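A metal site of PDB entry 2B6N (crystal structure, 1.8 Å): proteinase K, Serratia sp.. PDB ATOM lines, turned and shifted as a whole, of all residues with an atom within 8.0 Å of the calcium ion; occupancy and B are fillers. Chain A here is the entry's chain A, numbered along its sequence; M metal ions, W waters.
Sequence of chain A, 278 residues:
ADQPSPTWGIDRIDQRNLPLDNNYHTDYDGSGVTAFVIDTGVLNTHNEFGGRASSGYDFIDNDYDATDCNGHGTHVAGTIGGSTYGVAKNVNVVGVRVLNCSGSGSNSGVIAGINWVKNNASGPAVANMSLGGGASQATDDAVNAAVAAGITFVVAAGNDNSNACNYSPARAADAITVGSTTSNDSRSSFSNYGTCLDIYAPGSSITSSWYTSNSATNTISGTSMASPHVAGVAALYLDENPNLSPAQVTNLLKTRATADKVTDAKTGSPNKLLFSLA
Water W1 bridges the side-chain carboxylate of Asp 21 (2.5 Å) and the side-chain carboxylate of Asp 14 (3.3 Å).
The calcium ion is bound by the side-chain carboxylate of Asp 14, the backbone carbonyl oxygen of Asn 23, the backbone carbonyl oxygen of Asp 11, the side-chain carboxylate of Asp 11, the side-chain amide oxygen of Gln 15, the side-chain carboxylate of Asp 21 and water W1.
The backbone carbonyl oxygen (O) of Pro 19 lies within hydrogen-bond range of the side-chain amide nitrogen (NE2) of Gln 15 (2.9 Å).
O of Gln 15 sits at hydrogen-bond distance from NH1 of Arg 12, 2.9 Å away.
NE2 of Gln 15 lies within hydrogen-bond range of O of Asn 17, at 2.7 Å.
OD2 of Asp 14 is in hydrogen-bond range of N of His 25, 2.7 Å away.
The side-chain carboxylate of Asp 11 lies within hydrogen-bond range of the backbone NH of Asn 22 (2.9 Å).
The side-chain amide nitrogen of Asn 23 sits close to the backbone carbonyl oxygen of Gln 3, at 3.4 Å.
Five residues have an atom within 4 Å of the calcium ion: Asp 11, Asp 14, Gln 15, Asp 21 and Asn 23.
The nearest printed residue that does not touch the calcium ion is Arg 12 (4.6 Å).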
ATOM      1  N   GLN A   3      -0.598   7.050  22.950  1.00  0.00           N
ATOM      2  CA  GLN A   3      -0.701   5.920  22.052  1.00  0.00           C
ATOM      3  C   GLN A   3      -0.719   4.633  22.888  1.00  0.00           C
ATOM      4  O   GLN A   3       0.260   4.336  23.567  1.00  0.00           O
ATOM      5  CB  GLN A   3       0.451   5.899  21.027  1.00  0.00           C
ATOM      6  CG  GLN A   3       0.564   4.555  20.320  1.00  0.00           C
ATOM      7  CD  GLN A   3       1.694   4.511  19.302  1.00  0.00           C
ATOM      8  OE1 GLN A   3       2.638   5.309  19.364  1.00  0.00           O
ATOM      9  NE2 GLN A   3       1.619   3.553  18.369  1.00  0.00           N
ATOM     10  N   PRO A   6       1.953   0.603  22.300  1.00  0.00           N
ATOM     11  CA  PRO A   6       3.065   0.900  21.408  1.00  0.00           C
ATOM     12  C   PRO A   6       4.076  -0.236  21.417  1.00  0.00           C
ATOM     13  O   PRO A   6       4.068  -1.063  22.332  1.00  0.00           O
ATOM     14  CB  PRO A   6       3.663   2.167  22.034  1.00  0.00           C
ATOM     15  CG  PRO A   6       3.447   1.979  23.492  1.00  0.00           C
ATOM     16  CD  PRO A   6       2.069   1.333  23.578  1.00  0.00           C
ATOM     17  N   THR A   7       4.933  -0.288  20.392  1.00  0.00           N
ATOM     18  CA  THR A   7       6.073  -1.188  20.419  1.00  0.00           C
ATOM     19  C   THR A   7       6.971  -0.780  21.601  1.00  0.00           C
ATOM     20  O   THR A   7       6.875   0.352  22.078  1.00  0.00           O
ATOM     21  CB  THR A   7       6.797  -1.177  19.052  1.00  0.00           C
ATOM     22  OG1 THR A   7       7.726  -2.262  19.005  1.00  0.00           O
ATOM     23  CG2 THR A   7       7.491   0.188  18.786  1.00  0.00           C
ATOM     24  N   TRP A   8       7.805  -1.708  22.088  1.00  0.00           N
ATOM     25  CA  TRP A   8       8.489  -1.523  23.383  1.00  0.00           C
ATOM     26  C   TRP A   8       9.442  -0.351  23.436  1.00  0.00           C
ATOM     27  O   TRP A   8       9.524   0.311  24.467  1.00  0.00           O
ATOM     28  CB  TRP A   8       9.179  -2.824  23.880  1.00  0.00           C
ATOM     29  CG  TRP A   8      10.620  -3.020  23.465  1.00  0.00           C
ATOM     30  CD1 TRP A   8      11.070  -3.767  22.394  1.00  0.00           C
ATOM     31  CD2 TRP A   8      11.793  -2.467  24.088  1.00  0.00           C
ATOM     32  NE1 TRP A   8      12.438  -3.743  22.348  1.00  0.00           N
ATOM     33  CE2 TRP A   8      12.912  -2.926  23.357  1.00  0.00           C
ATOM     34  CE3 TRP A   8      12.001  -1.619  25.195  1.00  0.00           C
ATOM     35  CZ2 TRP A   8      14.231  -2.596  23.706  1.00  0.00           C
ATOM     36  CZ3 TRP A   8      13.317  -1.267  25.522  1.00  0.00           C
ATOM     37  CH2 TRP A   8      14.425  -1.761  24.771  1.00  0.00           C
ATOM     38  N   GLY A   9      10.171  -0.109  22.343  1.00  0.00           N
ATOM     39  CA  GLY A   9      11.187   0.956  22.326  1.00  0.00           C
ATOM     40  C   GLY A   9      10.609   2.299  22.698  1.00  0.00           C
ATOM     41  O   GLY A   9      11.063   2.952  23.663  1.00  0.00           O
ATOM     42  N   ILE A  10       9.608   2.737  21.920  1.00  0.00           N
ATOM     43  CA  ILE A  10       8.956   4.012  22.185  1.00  0.00           C
ATOM     44  C   ILE A  10       8.185   3.983  23.522  1.00  0.00           C
ATOM     45  O   ILE A  10       8.122   4.991  24.211  1.00  0.00           O
ATOM     46  CB  ILE A  10       8.079   4.511  20.992  1.00  0.00           C
ATOM     47  CG1 ILE A  10       6.874   3.588  20.752  1.00  0.00           C
ATOM     48  CG2 ILE A  10       8.935   4.663  19.717  1.00  0.00           C
ATOM     49  CD1 ILE A  10       5.995   4.054  19.588  1.00  0.00           C
ATOM     50  N   ASP A  11       7.627   2.823  23.899  1.00  0.00           N
ATOM     51  CA  ASP A  11       7.013   2.654  25.244  1.00  0.00           C
ATOM     52  C   ASP A  11       8.010   3.023  26.376  1.00  0.00           C
ATOM     53  O   ASP A  11       7.647   3.645  27.393  1.00  0.00           O
ATOM     54  CB  ASP A  11       6.519   1.195  25.411  1.00  0.00           C
ATOM     55  CG  ASP A  11       5.513   1.018  26.579  1.00  0.00           C
ATOM     56  OD1 ASP A  11       5.225   1.980  27.330  1.00  0.00           O
ATOM     57  OD2 ASP A  11       5.017  -0.119  26.718  1.00  0.00           O
ATOM     58  N   ARG A  12       9.269   2.627  26.195  1.00  0.00           N
ATOM     59  CA  ARG A  12      10.299   2.846  27.215  1.00  0.00           C
ATOM     60  C   ARG A  12      10.708   4.294  27.427  1.00  0.00           C
ATOM     61  O   ARG A  12      10.986   4.703  28.564  1.00  0.00           O
ATOM     62  CB  ARG A  12      11.556   2.016  26.904  1.00  0.00           C
ATOM     63  CG  ARG A  12      12.709   2.143  27.970  1.00  0.00           C
ATOM     64  CD  ARG A  12      12.344   1.330  29.228  1.00  0.00           C
ATOM     65  NE  ARG A  12      13.177   1.583  30.421  1.00  0.00           N
ATOM     66  CZ  ARG A  12      13.021   2.599  31.269  1.00  0.00           C
ATOM     67  NH1 ARG A  12      12.124   3.557  31.046  1.00  0.00           N
ATOM     68  NH2 ARG A  12      13.805   2.680  32.332  1.00  0.00           N
ATOM     69  N   ILE A  13      10.740   5.073  26.346  1.00  0.00           N
ATOM     70  CA  ILE A  13      11.390   6.388  26.370  1.00  0.00           C
ATOM     71  C   ILE A  13      10.573   7.466  27.103  1.00  0.00           C
ATOM     72  O   ILE A  13      11.144   8.439  27.607  1.00  0.00           O
ATOM     73  CB  ILE A  13      11.836   6.822  24.942  1.00  0.00           C
ATOM     74  CG1 ILE A  13      12.814   5.805  24.349  1.00  0.00           C
ATOM     75  CG2 ILE A  13      12.482   8.195  24.971  1.00  0.00           C
ATOM     76  CD1 ILE A  13      14.047   5.557  25.194  1.00  0.00           C
ATOM     77  N   ASP A  14       9.253   7.283  27.208  1.00  0.00           N
ATOM     78  CA  ASP A  14       8.381   8.285  27.885  1.00  0.00           C
ATOM     79  C   ASP A  14       8.150   8.047  29.393  1.00  0.00           C
ATOM     80  O   ASP A  14       7.255   8.660  30.009  1.00  0.00           O
ATOM     81  CB  ASP A  14       7.027   8.458  27.136  1.00  0.00           C
ATOM     82  CG  ASP A  14       6.062   7.329  27.427  1.00  0.00           C
ATOM     83  OD1 ASP A  14       6.509   6.210  27.761  1.00  0.00           O
ATOM     84  OD2 ASP A  14       4.849   7.594  27.383  1.00  0.00           O
ATOM     85  N   GLN A  15       8.970   7.189  30.004  1.00  0.00           N
ATOM     86  CA  GLN A  15       8.869   6.871  31.430  1.00  0.00           C
ATOM     87  C   GLN A  15      10.249   6.663  32.048  1.00  0.00           C
ATOM     88  O   GLN A  15      11.203   6.265  31.348  1.00  0.00           O
ATOM     89  CB  GLN A  15       7.968   5.633  31.624  1.00  0.00           C
ATOM     90  CG  GLN A  15       8.422   4.395  30.830  1.00  0.00           C
ATOM     91  CD  GLN A  15       7.482   3.232  31.003  1.00  0.00           C
ATOM     92  OE1 GLN A  15       6.548   3.061  30.213  1.00  0.00           O
ATOM     93  NE2 GLN A  15       7.713   2.424  32.043  1.00  0.00           N
ATOM     94  N   ARG A  16      10.364   6.880  33.362  1.00  0.00           N
ATOM     95  CA  ARG A  16      11.668   6.746  34.058  1.00  0.00           C
ATOM     96  C   ARG A  16      12.004   5.293  34.401  1.00  0.00           C
ATOM     97  O   ARG A  16      13.124   4.817  34.202  1.00  0.00           O
ATOM     98  CB  ARG A  16      11.678   7.576  35.354  1.00  0.00           C
ATOM     99  CG  ARG A  16      11.385   9.068  35.139  1.00  0.00           C
ATOM    100  CD  ARG A  16      12.507   9.686  34.303  1.00  0.00           C
ATOM    101  NE  ARG A  16      12.436  11.133  34.215  1.00  0.00           N
ATOM    102  CZ  ARG A  16      13.280  11.887  33.494  1.00  0.00           C
ATOM    103  NH1 ARG A  16      14.237  11.310  32.781  1.00  0.00           N
ATOM    104  NH2 ARG A  16      13.130  13.218  33.478  1.00  0.00           N
ATOM    105  N   ASN A  17      10.999   4.604  34.940  1.00  0.00           N
ATOM    106  CA  ASN A  17      11.168   3.280  35.525  1.00  0.00           C
ATOM    107  C   ASN A  17      10.400   2.212  34.768  1.00  0.00           C
ATOM    108  O   ASN A  17       9.329   2.499  34.205  1.00  0.00           O
ATOM    109  CB  ASN A  17      10.673   3.287  36.981  1.00  0.00           C
ATOM    110  CG  ASN A  17      11.284   4.405  37.798  1.00  0.00           C
ATOM    111  OD1 ASN A  17      12.503   4.572  37.810  1.00  0.00           O
ATOM    112  ND2 ASN A  17      10.457   5.164  38.488  1.00  0.00           N
ATOM    113  N   PRO A  19       8.187  -1.328  35.266  1.00  0.00           N
ATOM    114  CA  PRO A  19       7.872  -1.997  33.982  1.00  0.00           C
ATOM    115  C   PRO A  19       7.247  -1.074  32.925  1.00  0.00           C
ATOM    116  O   PRO A  19       6.754   0.005  33.249  1.00  0.00           O
ATOM    117  CB  PRO A  19       6.872  -3.079  34.405  1.00  0.00           C
ATOM    118  CG  PRO A  19       6.135  -2.446  35.544  1.00  0.00           C
ATOM    119  CD  PRO A  19       7.170  -1.643  36.298  1.00  0.00           C
ATOM    120  N   LEU A  20       7.289  -1.522  31.671  1.00  0.00           N
ATOM    121  CA  LEU A  20       6.640  -0.791  30.564  1.00  0.00           C
ATOM    122  C   LEU A  20       5.145  -0.657  30.880  1.00  0.00           C
ATOM    123  O   LEU A  20       4.536  -1.604  31.359  1.00  0.00           O
ATOM    124  CB  LEU A  20       6.836  -1.568  29.248  1.00  0.00           C
ATOM    125  CG  LEU A  20       8.301  -1.656  28.794  1.00  0.00           C
ATOM    126  CD1 LEU A  20       8.446  -2.556  27.558  1.00  0.00           C
ATOM    127  CD2 LEU A  20       8.867  -0.247  28.555  1.00  0.00           C
ATOM    128  N   ASP A  21       4.579   0.526  30.650  1.00  0.00           N
ATOM    129  CA  ASP A  21       3.147   0.767  30.907  1.00  0.00           C
ATOM    130  C   ASP A  21       2.219   0.670  29.674  1.00  0.00           C
ATOM    131  O   ASP A  21       1.042   1.003  29.756  1.00  0.00           O
ATOM    132  CB  ASP A  21       2.954   2.103  31.647  1.00  0.00           C
ATOM    133  CG  ASP A  21       3.187   3.327  30.768  1.00  0.00           C
ATOM    134  OD1 ASP A  21       3.637   3.218  29.605  1.00  0.00           O
ATOM    135  OD2 ASP A  21       2.906   4.444  31.258  1.00  0.00           O
ATOM    136  N   ASN A  22       2.741   0.191  28.538  1.00  0.00           N
ATOM    137  CA  ASN A  22       1.900  -0.016  27.343  1.00  0.00           C
ATOM    138  C   ASN A  22       1.273   1.283  26.828  1.00  0.00           C
ATOM    139  O   ASN A  22       0.133   1.296  26.324  1.00  0.00           O
ATOM    140  CB  ASN A  22       0.792  -1.044  27.644  1.00  0.00           C
ATOM    141  CG  ASN A  22       0.267  -1.726  26.386  1.00  0.00           C
ATOM    142  OD1 ASN A  22      -0.968  -1.794  26.135  1.00  0.00           O
ATOM    143  ND2 ASN A  22       1.168  -2.254  25.590  1.00  0.00           N
ATOM    144  N   ASN A  23       2.022   2.377  26.988  1.00  0.00           N
ATOM    145  CA  ASN A  23       1.585   3.696  26.596  1.00  0.00           C
ATOM    146  C   ASN A  23       2.754   4.553  26.100  1.00  0.00           C
ATOM    147  O   ASN A  23       3.817   4.576  26.748  1.00  0.00           O
ATOM    148  CB  ASN A  23       0.938   4.444  27.764  1.00  0.00           C
ATOM    149  CG  ASN A  23       0.181   5.684  27.295  1.00  0.00           C
ATOM    150  OD1 ASN A  23       0.574   6.817  27.577  1.00  0.00           O
ATOM    151  ND2 ASN A  23      -0.906   5.467  26.584  1.00  0.00           N
ATOM    152  N   TYR A  24       2.534   5.242  24.981  1.00  0.00           N
ATOM    153  CA  TYR A  24       3.520   6.223  24.492  1.00  0.00           C
ATOM    154  C   TYR A  24       2.862   7.606  24.440  1.00  0.00           C
ATOM    155  O   TYR A  24       2.048   7.898  23.557  1.00  0.00           O
ATOM    156  CB  TYR A  24       4.152   5.820  23.145  1.00  0.00           C
ATOM    157  CG  TYR A  24       5.112   6.892  22.629  1.00  0.00           C
ATOM    158  CD1 TYR A  24       6.172   7.339  23.428  1.00  0.00           C
ATOM    159  CD2 TYR A  24       4.946   7.471  21.376  1.00  0.00           C
ATOM    160  CE1 TYR A  24       7.045   8.324  22.997  1.00  0.00           C
ATOM    161  CE2 TYR A  24       5.837   8.466  20.917  1.00  0.00           C
ATOM    162  CZ  TYR A  24       6.867   8.903  21.750  1.00  0.00           C
ATOM    163  OH  TYR A  24       7.739   9.889  21.333  1.00  0.00           O
ATOM    164  N   HIS A  25       3.206   8.435  25.427  1.00  0.00           N
ATOM    165  CA  HIS A  25       2.663   9.788  25.510  1.00  0.00           C
ATOM    166  C   HIS A  25       3.499  10.733  24.681  1.00  0.00           C
ATOM    167  O   HIS A  25       4.728  10.640  24.684  1.00  0.00           O
ATOM    168  CB  HIS A  25       2.648  10.262  26.970  1.00  0.00           C
ATOM    169  CG  HIS A  25       2.129  11.647  27.145  1.00  0.00           C
ATOM    170  ND1 HIS A  25       0.796  11.922  27.299  1.00  0.00           N
ATOM    171  CD2 HIS A  25       2.765  12.840  27.167  1.00  0.00           C
ATOM    172  CE1 HIS A  25       0.621  13.235  27.388  1.00  0.00           C
ATOM    173  NE2 HIS A  25       1.801  13.815  27.309  1.00  0.00           N
HETATM  174 CA    CA M   1       5.526   4.145  28.320  1.00  0.00          CA
HETATM  175  O   HOH W   1       4.708   5.812  30.098  1.00  0.00           O
